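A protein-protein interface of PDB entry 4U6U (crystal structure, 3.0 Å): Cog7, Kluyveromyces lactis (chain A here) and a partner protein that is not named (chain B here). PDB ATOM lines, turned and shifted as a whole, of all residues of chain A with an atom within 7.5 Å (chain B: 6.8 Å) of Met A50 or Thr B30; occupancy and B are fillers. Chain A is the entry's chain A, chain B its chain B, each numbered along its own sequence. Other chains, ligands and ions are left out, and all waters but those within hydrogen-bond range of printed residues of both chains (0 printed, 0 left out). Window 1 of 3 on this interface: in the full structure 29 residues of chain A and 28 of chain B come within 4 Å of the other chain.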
ATOM      1  N   LEU A   9      -6.038   7.211  -8.068  1.00  0.00           N
ATOM      2  CA  LEU A   9      -4.960   8.180  -8.242  1.00  0.00           C
ATOM      3  C   LEU A   9      -3.665   7.485  -8.557  1.00  0.00           C
ATOM      4  O   LEU A   9      -2.984   7.867  -9.498  1.00  0.00           O
ATOM      5  CB  LEU A   9      -4.782   9.030  -6.986  1.00  0.00           C
ATOM      6  CG  LEU A   9      -4.436  10.499  -7.178  1.00  0.00           C
ATOM      7  CD1 LEU A   9      -3.109  10.806  -6.513  1.00  0.00           C
ATOM      8  CD2 LEU A   9      -4.412  10.845  -8.668  1.00  0.00           C
ATOM      9  N   MET A  12      -4.082   5.385 -11.961  1.00  0.00           N
ATOM     10  CA  MET A  12      -4.093   6.289 -13.079  1.00  0.00           C
ATOM     11  C   MET A  12      -2.714   6.402 -13.664  1.00  0.00           C
ATOM     12  O   MET A  12      -2.529   6.346 -14.867  1.00  0.00           O
ATOM     13  CB  MET A  12      -4.616   7.636 -12.614  1.00  0.00           C
ATOM     14  CG  MET A  12      -4.102   8.843 -13.343  1.00  0.00           C
ATOM     15  SD  MET A  12      -4.744  10.289 -12.497  1.00  0.00           S
ATOM     16  CE  MET A  12      -6.508   9.920 -12.580  1.00  0.00           C
ATOM     17  N   PHE A  13      -1.730   6.520 -12.790  1.00  0.00           N
ATOM     18  CA  PHE A  13      -0.352   6.656 -13.212  1.00  0.00           C
ATOM     19  C   PHE A  13       0.223   5.406 -13.865  1.00  0.00           C
ATOM     20  O   PHE A  13       1.203   5.480 -14.587  1.00  0.00           O
ATOM     21  CB  PHE A  13       0.508   7.011 -12.028  1.00  0.00           C
ATOM     22  CG  PHE A  13       0.360   8.410 -11.574  1.00  0.00           C
ATOM     23  CD1 PHE A  13       0.645   9.457 -12.430  1.00  0.00           C
ATOM     24  CD2 PHE A  13       0.040   8.691 -10.259  1.00  0.00           C
ATOM     25  CE1 PHE A  13       0.557  10.752 -11.994  1.00  0.00           C
ATOM     26  CE2 PHE A  13      -0.043  10.002  -9.820  1.00  0.00           C
ATOM     27  CZ  PHE A  13       0.221  11.024 -10.684  1.00  0.00           C
ATOM     28  N   PHE A  18      -1.700   7.296 -20.017  1.00  0.00           N
ATOM     29  CA  PHE A  18      -1.808   8.429 -19.119  1.00  0.00           C
ATOM     30  C   PHE A  18      -0.830   9.481 -19.577  1.00  0.00           C
ATOM     31  O   PHE A  18       0.374   9.240 -19.647  1.00  0.00           O
ATOM     32  CB  PHE A  18      -1.524   8.080 -17.648  1.00  0.00           C
ATOM     33  CG  PHE A  18      -1.444   9.307 -16.754  1.00  0.00           C
ATOM     34  CD1 PHE A  18      -2.586   9.870 -16.218  1.00  0.00           C
ATOM     35  CD2 PHE A  18      -0.224   9.916 -16.484  1.00  0.00           C
ATOM     36  CE1 PHE A  18      -2.523  10.994 -15.434  1.00  0.00           C
ATOM     37  CE2 PHE A  18      -0.153  11.056 -15.688  1.00  0.00           C
ATOM     38  CZ  PHE A  18      -1.303  11.595 -15.165  1.00  0.00           C
ATOM     39  N   VAL A  19      -1.336  10.659 -19.885  1.00  0.00           N
ATOM     40  CA  VAL A  19      -0.434  11.725 -20.268  1.00  0.00           C
ATOM     41  C   VAL A  19      -0.544  12.893 -19.275  1.00  0.00           C
ATOM     42  O   VAL A  19      -1.628  13.432 -19.064  1.00  0.00           O
ATOM     43  CB  VAL A  19      -0.703  12.164 -21.745  1.00  0.00           C
ATOM     44  CG1 VAL A  19      -2.092  11.711 -22.216  1.00  0.00           C
ATOM     45  CG2 VAL A  19      -0.499  13.647 -21.904  1.00  0.00           C
ATOM     46  N   PRO A  20       0.575  13.247 -18.615  1.00  0.00           N
ATOM     47  CA  PRO A  20       0.584  14.300 -17.590  1.00  0.00           C
ATOM     48  C   PRO A  20       0.044  15.642 -18.076  1.00  0.00           C
ATOM     49  O   PRO A  20      -0.792  16.212 -17.374  1.00  0.00           O
ATOM     50  CB  PRO A  20       2.062  14.414 -17.213  1.00  0.00           C
ATOM     51  CG  PRO A  20       2.605  13.080 -17.472  1.00  0.00           C
ATOM     52  CD  PRO A  20       1.871  12.552 -18.684  1.00  0.00           C
ATOM     53  N   GLN A  21       0.475  16.124 -19.240  1.00  0.00           N
ATOM     54  CA  GLN A  21      -0.041  17.394 -19.752  1.00  0.00           C
ATOM     55  C   GLN A  21      -1.575  17.392 -19.817  1.00  0.00           C
ATOM     56  O   GLN A  21      -2.227  18.406 -19.584  1.00  0.00           O
ATOM     57  CB  GLN A  21       0.551  17.706 -21.131  1.00  0.00           C
ATOM     58  CG  GLN A  21       1.734  18.679 -21.125  1.00  0.00           C
ATOM     59  CD  GLN A  21       1.303  20.133 -21.166  1.00  0.00           C
ATOM     60  OE1 GLN A  21       0.218  20.489 -20.714  1.00  0.00           O
ATOM     61  NE2 GLN A  21       2.152  20.977 -21.723  1.00  0.00           N
ATOM     62  N   PHE A  23      -3.755  15.459 -17.978  1.00  0.00           N
ATOM     63  CA  PHE A  23      -4.428  15.316 -16.696  1.00  0.00           C
ATOM     64  C   PHE A  23      -4.622  16.630 -15.967  1.00  0.00           C
ATOM     65  O   PHE A  23      -5.712  16.915 -15.457  1.00  0.00           O
ATOM     66  CB  PHE A  23      -3.662  14.363 -15.772  1.00  0.00           C
ATOM     67  CG  PHE A  23      -4.180  14.376 -14.359  1.00  0.00           C
ATOM     68  CD1 PHE A  23      -5.276  13.608 -14.013  1.00  0.00           C
ATOM     69  CD2 PHE A  23      -3.601  15.184 -13.387  1.00  0.00           C
ATOM     70  CE1 PHE A  23      -5.781  13.633 -12.723  1.00  0.00           C
ATOM     71  CE2 PHE A  23      -4.111  15.215 -12.105  1.00  0.00           C
ATOM     72  CZ  PHE A  23      -5.202  14.435 -11.775  1.00  0.00           C
ATOM     73  N   VAL A  24      -3.547  17.405 -15.894  1.00  0.00           N
ATOM     74  CA  VAL A  24      -3.550  18.689 -15.200  1.00  0.00           C
ATOM     75  C   VAL A  24      -4.522  19.632 -15.910  1.00  0.00           C
ATOM     76  O   VAL A  24      -5.199  20.452 -15.279  1.00  0.00           O
ATOM     77  CB  VAL A  24      -2.137  19.310 -15.149  1.00  0.00           C
ATOM     78  CG1 VAL A  24      -2.154  20.591 -14.360  1.00  0.00           C
ATOM     79  CG2 VAL A  24      -1.184  18.365 -14.482  1.00  0.00           C
ATOM     80  N   LEU A  27      -8.030  18.963 -14.999  1.00  0.00           N
ATOM     81  CA  LEU A  27      -8.211  19.214 -13.579  1.00  0.00           C
ATOM     82  C   LEU A  27      -8.485  20.677 -13.266  1.00  0.00           C
ATOM     83  O   LEU A  27      -9.548  21.026 -12.741  1.00  0.00           O
ATOM     84  CB  LEU A  27      -6.976  18.733 -12.807  1.00  0.00           C
ATOM     85  CG  LEU A  27      -6.929  19.158 -11.339  1.00  0.00           C
ATOM     86  CD1 LEU A  27      -8.079  18.534 -10.589  1.00  0.00           C
ATOM     87  CD2 LEU A  27      -5.594  18.810 -10.679  1.00  0.00           C
ATOM     88  N   CYS A  43      -5.634  21.689  -5.131  1.00  0.00           N
ATOM     89  CA  CYS A  43      -4.380  21.233  -5.716  1.00  0.00           C
ATOM     90  C   CYS A  43      -3.253  21.036  -4.713  1.00  0.00           C
ATOM     91  O   CYS A  43      -2.388  20.189  -4.925  1.00  0.00           O
ATOM     92  CB  CYS A  43      -3.918  22.201  -6.797  1.00  0.00           C
ATOM     93  SG  CYS A  43      -4.888  22.055  -8.283  1.00  0.00           S
ATOM     94  N   SER A  44      -3.236  21.820  -3.642  1.00  0.00           N
ATOM     95  CA  SER A  44      -2.221  21.620  -2.619  1.00  0.00           C
ATOM     96  C   SER A  44      -2.263  20.203  -2.069  1.00  0.00           C
ATOM     97  O   SER A  44      -1.233  19.538  -2.004  1.00  0.00           O
ATOM     98  CB  SER A  44      -2.378  22.617  -1.467  1.00  0.00           C
ATOM     99  OG  SER A  44      -1.685  23.827  -1.725  1.00  0.00           O
ATOM    100  N   SER A  45      -3.449  19.763  -1.662  1.00  0.00           N
ATOM    101  CA  SER A  45      -3.635  18.441  -1.068  1.00  0.00           C
ATOM    102  C   SER A  45      -3.370  17.332  -2.081  1.00  0.00           C
ATOM    103  O   SER A  45      -2.682  16.342  -1.796  1.00  0.00           O
ATOM    104  CB  SER A  45      -5.046  18.305  -0.493  1.00  0.00           C
ATOM    105  OG  SER A  45      -6.006  18.236  -1.535  1.00  0.00           O
ATOM    106  N   LEU A  46      -3.957  17.491  -3.255  1.00  0.00           N
ATOM    107  CA  LEU A  46      -3.762  16.562  -4.345  1.00  0.00           C
ATOM    108  C   LEU A  46      -2.255  16.390  -4.601  1.00  0.00           C
ATOM    109  O   LEU A  46      -1.779  15.288  -4.809  1.00  0.00           O
ATOM    110  CB  LEU A  46      -4.512  17.070  -5.568  1.00  0.00           C
ATOM    111  CG  LEU A  46      -4.761  16.131  -6.730  1.00  0.00           C
ATOM    112  CD1 LEU A  46      -3.592  16.185  -7.702  1.00  0.00           C
ATOM    113  CD2 LEU A  46      -5.001  14.730  -6.178  1.00  0.00           C
ATOM    114  N   LEU A  47      -1.506  17.487  -4.583  1.00  0.00           N
ATOM    115  CA  LEU A  47      -0.041  17.436  -4.660  1.00  0.00           C
ATOM    116  C   LEU A  47       0.615  16.587  -3.531  1.00  0.00           C
ATOM    117  O   LEU A  47       1.585  15.880  -3.751  1.00  0.00           O
ATOM    118  CB  LEU A  47       0.515  18.857  -4.652  1.00  0.00           C
ATOM    119  CG  LEU A  47       1.396  19.307  -5.824  1.00  0.00           C
ATOM    120  CD1 LEU A  47       1.247  18.465  -7.078  1.00  0.00           C
ATOM    121  CD2 LEU A  47       1.085  20.748  -6.155  1.00  0.00           C
ATOM    122  N   SER A  48       0.083  16.659  -2.321  1.00  0.00           N
ATOM    123  CA  SER A  48       0.696  15.966  -1.214  1.00  0.00           C
ATOM    124  C   SER A  48       0.615  14.463  -1.398  1.00  0.00           C
ATOM    125  O   SER A  48       1.440  13.704  -0.903  1.00  0.00           O
ATOM    126  CB  SER A  48       0.016  16.372   0.079  1.00  0.00           C
ATOM    127  OG  SER A  48       0.544  17.609   0.493  1.00  0.00           O
ATOM    128  N   LYS A  49      -0.338  14.042  -2.197  1.00  0.00           N
ATOM    129  CA  LYS A  49      -0.766  12.669  -2.183  1.00  0.00           C
ATOM    130  C   LYS A  49       0.064  12.106  -3.309  1.00  0.00           C
ATOM    131  O   LYS A  49       0.661  11.039  -3.203  1.00  0.00           O
ATOM    132  CB  LYS A  49      -2.268  12.576  -2.430  1.00  0.00           C
ATOM    133  CG  LYS A  49      -2.966  11.243  -2.202  1.00  0.00           C
ATOM    134  CD  LYS A  49      -4.478  11.474  -2.420  1.00  0.00           C
ATOM    135  CE  LYS A  49      -5.395  10.328  -1.983  1.00  0.00           C
ATOM    136  NZ  LYS A  49      -5.233   9.057  -2.746  1.00  0.00           N
ATOM    137  N   MET A  50       0.134  12.873  -4.384  1.00  0.00           N
ATOM    138  CA  MET A  50       1.056  12.582  -5.451  1.00  0.00           C
ATOM    139  C   MET A  50       2.467  12.510  -4.907  1.00  0.00           C
ATOM    140  O   MET A  50       3.257  11.640  -5.293  1.00  0.00           O
ATOM    141  CB  MET A  50       0.919  13.616  -6.560  1.00  0.00           C
ATOM    142  CG  MET A  50      -0.331  13.332  -7.383  1.00  0.00           C
ATOM    143  SD  MET A  50      -0.651  14.608  -8.576  1.00  0.00           S
ATOM    144  CE  MET A  50       1.047  14.872  -9.085  1.00  0.00           C
ATOM    145  N   ASP A  51       2.786  13.411  -3.996  1.00  0.00           N
ATOM    146  CA  ASP A  51       4.096  13.342  -3.395  1.00  0.00           C
ATOM    147  C   ASP A  51       4.326  12.016  -2.674  1.00  0.00           C
ATOM    148  O   ASP A  51       5.368  11.395  -2.878  1.00  0.00           O
ATOM    149  CB  ASP A  51       4.315  14.499  -2.446  1.00  0.00           C
ATOM    150  CG  ASP A  51       4.792  15.719  -3.158  1.00  0.00           C
ATOM    151  OD1 ASP A  51       5.188  15.572  -4.350  1.00  0.00           O
ATOM    152  OD2 ASP A  51       4.806  16.792  -2.517  1.00  0.00           O
ATOM    153  N   TYR A  52       3.354  11.567  -1.878  1.00  0.00           N
ATOM    154  CA  TYR A  52       3.477  10.290  -1.177  1.00  0.00           C
ATOM    155  C   TYR A  52       3.722   9.157  -2.186  1.00  0.00           C
ATOM    156  O   TYR A  52       4.629   8.348  -2.034  1.00  0.00           O
ATOM    157  CB  TYR A  52       2.225   9.980  -0.363  1.00  0.00           C
ATOM    158  CG  TYR A  52       2.245   8.595   0.201  1.00  0.00           C
ATOM    159  CD1 TYR A  52       2.882   8.340   1.359  1.00  0.00           C
ATOM    160  CD2 TYR A  52       1.677   7.525  -0.482  1.00  0.00           C
ATOM    161  CE1 TYR A  52       2.932   7.093   1.870  1.00  0.00           C
ATOM    162  CE2 TYR A  52       1.727   6.227   0.041  1.00  0.00           C
ATOM    163  CZ  TYR A  52       2.367   6.024   1.223  1.00  0.00           C
ATOM    164  OH  TYR A  52       2.469   4.758   1.801  1.00  0.00           O
ATOM    165  N   TYR A  53       2.893   9.119  -3.216  1.00  0.00           N
ATOM    166  CA  TYR A  53       2.985   8.114  -4.250  1.00  0.00           C
ATOM    167  C   TYR A  53       4.340   8.154  -4.931  1.00  0.00           C
ATOM    168  O   TYR A  53       4.950   7.120  -5.215  1.00  0.00           O
ATOM    169  CB  TYR A  53       1.843   8.319  -5.269  1.00  0.00           C
ATOM    170  CG  TYR A  53       0.530   7.827  -4.712  1.00  0.00           C
ATOM    171  CD1 TYR A  53       0.493   6.703  -3.898  1.00  0.00           C
ATOM    172  CD2 TYR A  53      -0.654   8.488  -4.965  1.00  0.00           C
ATOM    173  CE1 TYR A  53      -0.685   6.236  -3.375  1.00  0.00           C
ATOM    174  CE2 TYR A  53      -1.849   8.034  -4.428  1.00  0.00           C
ATOM    175  CZ  TYR A  53      -1.852   6.904  -3.634  1.00  0.00           C
ATOM    176  OH  TYR A  53      -3.019   6.412  -3.098  1.00  0.00           O
ATOM    177  N   SER A  54       4.832   9.352  -5.172  1.00  0.00           N
ATOM    178  CA  SER A  54       6.135   9.459  -5.785  1.00  0.00           C
ATOM    179  C   SER A  54       7.234   8.687  -5.013  1.00  0.00           C
ATOM    180  O   SER A  54       8.037   7.941  -5.604  1.00  0.00           O
ATOM    181  CB  SER A  54       6.515  10.913  -5.889  1.00  0.00           C
ATOM    182  OG  SER A  54       7.889  10.987  -6.111  1.00  0.00           O
ATOM    183  N   GLY A  55       7.223   8.824  -3.692  1.00  0.00           N
ATOM    184  CA  GLY A  55       8.213   8.189  -2.848  1.00  0.00           C
ATOM    185  C   GLY A  55       7.976   6.716  -2.649  1.00  0.00           C
ATOM    186  O   GLY A  55       8.912   5.944  -2.409  1.00  0.00           O
ATOM    187  N   HIS A  56       6.702   6.346  -2.698  1.00  0.00           N
ATOM    188  CA  HIS A  56       6.284   4.969  -2.630  1.00  0.00           C
ATOM    189  C   HIS A  56       6.828   4.290  -3.861  1.00  0.00           C
ATOM    190  O   HIS A  56       7.440   3.220  -3.774  1.00  0.00           O
ATOM    191  CB  HIS A  56       4.759   4.855  -2.550  1.00  0.00           C
ATOM    192  CG  HIS A  56       4.245   3.449  -2.673  1.00  0.00           C
ATOM    193  ND1 HIS A  56       4.394   2.516  -1.674  1.00  0.00           N
ATOM    194  CD2 HIS A  56       3.579   2.827  -3.670  1.00  0.00           C
ATOM    195  CE1 HIS A  56       3.874   1.365  -2.064  1.00  0.00           C
ATOM    196  NE2 HIS A  56       3.361   1.529  -3.269  1.00  0.00           N
ATOM    197  N   SER B  25       8.464   8.718 -13.663  1.00  0.00           N
ATOM    198  CA  SER B  25       8.553   9.881 -14.544  1.00  0.00           C
ATOM    199  C   SER B  25       7.216  10.553 -14.756  1.00  0.00           C
ATOM    200  O   SER B  25       7.132  11.762 -14.691  1.00  0.00           O
ATOM    201  CB  SER B  25       9.155   9.501 -15.870  1.00  0.00           C
ATOM    202  OG  SER B  25      10.534   9.269 -15.680  1.00  0.00           O
ATOM    203  N   LYS B  26       6.159   9.783 -14.965  1.00  0.00           N
ATOM    204  CA  LYS B  26       4.840  10.394 -15.104  1.00  0.00           C
ATOM    205  C   LYS B  26       4.437  11.151 -13.823  1.00  0.00           C
ATOM    206  O   LYS B  26       3.932  12.275 -13.924  1.00  0.00           O
ATOM    207  CB  LYS B  26       3.807   9.329 -15.492  1.00  0.00           C
ATOM    208  CG  LYS B  26       3.821   9.070 -17.003  1.00  0.00           C
ATOM    209  CD  LYS B  26       3.074   7.826 -17.424  1.00  0.00           C
ATOM    210  CE  LYS B  26       3.228   7.633 -18.918  1.00  0.00           C
ATOM    211  NZ  LYS B  26       2.856   6.251 -19.333  1.00  0.00           N
ATOM    212  N   ILE B  27       4.710  10.604 -12.630  1.00  0.00           N
ATOM    213  CA  ILE B  27       4.313  11.329 -11.417  1.00  0.00           C
ATOM    214  C   ILE B  27       5.093  12.638 -11.313  1.00  0.00           C
ATOM    215  O   ILE B  27       4.527  13.695 -11.008  1.00  0.00           O
ATOM    216  CB  ILE B  27       4.517  10.521 -10.142  1.00  0.00           C
ATOM    217  CG1 ILE B  27       3.551   9.336 -10.093  1.00  0.00           C
ATOM    218  CG2 ILE B  27       4.288  11.406  -8.915  1.00  0.00           C
ATOM    219  CD1 ILE B  27       3.762   8.463  -8.867  1.00  0.00           C
ATOM    220  N   HIS B  28       6.388  12.569 -11.601  1.00  0.00           N
ATOM    221  CA  HIS B  28       7.221  13.763 -11.562  1.00  0.00           C
ATOM    222  C   HIS B  28       6.765  14.874 -12.512  1.00  0.00           C
ATOM    223  O   HIS B  28       6.863  16.060 -12.189  1.00  0.00           O
ATOM    224  CB  HIS B  28       8.665  13.420 -11.883  1.00  0.00           C
ATOM    225  CG  HIS B  28       9.579  14.594 -11.761  1.00  0.00           C
ATOM    226  ND1 HIS B  28       9.967  15.104 -10.538  1.00  0.00           N
ATOM    227  CD2 HIS B  28      10.134  15.401 -12.693  1.00  0.00           C
ATOM    228  CE1 HIS B  28      10.753  16.146 -10.731  1.00  0.00           C
ATOM    229  NE2 HIS B  28      10.868  16.351 -12.033  1.00  0.00           N
ATOM    230  N   GLN B  29       6.305  14.491 -13.696  1.00  0.00           N
ATOM    231  CA  GLN B  29       5.885  15.468 -14.693  1.00  0.00           C
ATOM    232  C   GLN B  29       4.593  16.098 -14.232  1.00  0.00           C
ATOM    233  O   GLN B  29       4.409  17.319 -14.340  1.00  0.00           O
ATOM    234  CB  GLN B  29       5.715  14.821 -16.074  1.00  0.00           C
ATOM    235  CG  GLN B  29       6.984  14.141 -16.550  1.00  0.00           C
ATOM    236  CD  GLN B  29       6.824  13.379 -17.841  1.00  0.00           C
ATOM    237  OE1 GLN B  29       5.735  13.305 -18.408  1.00  0.00           O
ATOM    238  NE2 GLN B  29       7.905  12.744 -18.278  1.00  0.00           N
ATOM    239  N   THR B  30       3.702  15.255 -13.714  1.00  0.00           N
ATOM    240  CA  THR B  30       2.418  15.724 -13.233  1.00  0.00           C
ATOM    241  C   THR B  30       2.665  16.657 -12.072  1.00  0.00           C
ATOM    242  O   THR B  30       2.088  17.734 -11.967  1.00  0.00           O
ATOM    243  CB  THR B  30       1.503  14.556 -12.796  1.00  0.00           C
ATOM    244  OG1 THR B  30       1.423  13.598 -13.850  1.00  0.00           O
ATOM    245  CG2 THR B  30       0.071  15.043 -12.450  1.00  0.00           C
ATOM    246  N   THR B  31       3.573  16.255 -11.209  1.00  0.00           N
ATOM    247  CA  THR B  31       3.862  17.066 -10.057  1.00  0.00           C
ATOM    248  C   THR B  31       4.441  18.412 -10.471  1.00  0.00           C
ATOM    249  O   THR B  31       3.939  19.454 -10.036  1.00  0.00           O
ATOM    250  CB  THR B  31       4.806  16.317  -9.146  1.00  0.00           C
ATOM    251  OG1 THR B  31       4.022  15.753  -8.099  1.00  0.00           O
ATOM    252  CG2 THR B  31       5.966  17.228  -8.583  1.00  0.00           C
ATOM    253  N   THR B  32       5.424  18.395 -11.372  1.00  0.00           N
ATOM    254  CA  THR B  32       6.113  19.613 -11.726  1.00  0.00           C
ATOM    255  C   THR B  32       5.153  20.592 -12.373  1.00  0.00           C
ATOM    256  O   THR B  32       5.105  21.770 -12.009  1.00  0.00           O
ATOM    257  CB  THR B  32       7.258  19.370 -12.681  1.00  0.00           C
ATOM    258  OG1 THR B  32       8.203  18.470 -12.102  1.00  0.00           O
ATOM    259  CG2 THR B  32       7.947  20.686 -12.990  1.00  0.00           C
ATOM    260  N   LEU B  33       4.407  20.096 -13.352  1.00  0.00           N
ATOM    261  CA  LEU B  33       3.469  20.914 -14.078  1.00  0.00           C
ATOM    262  C   LEU B  33       2.453  21.537 -13.114  1.00  0.00           C
ATOM    263  O   LEU B  33       2.212  22.760 -13.120  1.00  0.00           O
ATOM    264  CB  LEU B  33       2.785  20.066 -15.152  1.00  0.00           C
ATOM    265  CG  LEU B  33       2.215  20.726 -16.413  1.00  0.00           C
ATOM    266  CD1 LEU B  33       0.759  21.092 -16.204  1.00  0.00           C
ATOM    267  CD2 LEU B  33       3.041  21.948 -16.803  1.00  0.00           C
ATOM    268  N   LEU B  34       1.897  20.700 -12.256  1.00  0.00           N
ATOM    269  CA  LEU B  34       0.910  21.156 -11.290  1.00  0.00           C
ATOM    270  C   LEU B  34       1.478  22.254 -10.374  1.00  0.00           C
ATOM    271  O   LEU B  34       0.800  23.230 -10.057  1.00  0.00           O
ATOM    272  CB  LEU B  34       0.404  19.960 -10.483  1.00  0.00           C
ATOM    273  CG  LEU B  34      -0.936  20.123  -9.783  1.00  0.00           C
ATOM    274  CD1 LEU B  34      -1.927  20.842 -10.670  1.00  0.00           C
ATOM    275  CD2 LEU B  34      -1.443  18.749  -9.426  1.00  0.00           C
ATOM    276  N   ARG B  35       2.728  22.107  -9.965  1.00  0.00           N
ATOM    277  CA  ARG B  35       3.335  23.124  -9.134  1.00  0.00           C
ATOM    278  C   ARG B  35       3.616  24.401  -9.926  1.00  0.00           C
ATOM    279  O   ARG B  35       3.417  25.489  -9.388  1.00  0.00           O
ATOM    280  CB  ARG B  35       4.622  22.609  -8.491  1.00  0.00           C
ATOM    281  CG  ARG B  35       4.393  21.660  -7.350  1.00  0.00           C
ATOM    282  CD  ARG B  35       5.546  21.686  -6.358  1.00  0.00           C
ATOM    283  NE  ARG B  35       5.126  21.015  -5.140  1.00  0.00           N
ATOM    284  CZ  ARG B  35       5.188  19.699  -4.971  1.00  0.00           C
ATOM    285  NH1 ARG B  35       5.649  18.920  -5.946  1.00  0.00           N
ATOM    286  NH2 ARG B  35       4.773  19.160  -3.837  1.00  0.00           N
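NH2 of Arg B35 is in salt-bridge range of OD2 of Asp A51 (2.7 Å).
The side-chain hydroxyl (OH) of Tyr A53 sits at hydrogen-bond distance from the side-chain amino group (NZ) of Lys A49 (3.5 Å). The side-chain hydroxyl (OG1) of Thr B30 sits at hydrogen-bond distance from the backbone carbonyl oxygen (O) of Lys B26.
CD2 of Phe A13 touches CG1 of Ile B27, 3.6 Å away. Phe A13 touches Thr B30 (CE1 to OG1, 3.5 Å). Phe A18 touches Thr B30 (CE2 to OG1, 3.5 Å). Pro A20 touches Lys B26 (CG to O, 3.9 Å). Thr B30 touches Phe A23 (CG2 to CD2, 3.8 Å). Val A24 touches Leu B33 (CG1 to CD1, 3.5 Å). Val A24 touches Leu B34. Leu B34 touches Leu A46 (CD2 to CD1, 3.8 Å). Ile B27 touches Met A50 (CG2 to O, 3.8 Å). OG1 of Thr B31 touches OD1 of Asp A51 (3.9 Å).
Printed residues of chain A within 4 Å of Thr B30: Phe A13 (3.5 Å), Phe A18 (3.5 Å), Pro A20 (3.5 Å), Phe A23 (3.8 Å) and Met A50 (3.5 Å). Printed residues of chain B within 4 Å of Ser A54: Ile B27 (3.8 Å). Of the printed residues of chain A, Gln B29 touches Pro A20. Printed residues of chain B within 4 Å of Phe A13: Ile B27 (3.6 Å) and Thr B30 (3.5 Å). Of the printed residues of chain A, Thr B31 touches Met A50 (3.3 Å) and Asp A51 (3.9 Å). Printed residues of chain B within 4 Å of Leu A47: Leu B34 and Arg B35. The nearest residue of chain B that does not touch Met A50 is Leu B34 (4.3 Å). The nearest printed residue of chain B that does not touch Phe A23 is Leu B34 (5.2 Å).
Of the 11 printed residues of chain B, 8 touch a printed residue of chain A. Hydrophobic or aromatic side chains of chain B that line the printed part of chain A: Ile B27, Leu B33 and Leu B34. Of the 24 printed residues of chain A, 12 touch a printed residue of chain B. Among the printed residues, 21 pairs touch across the chains.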
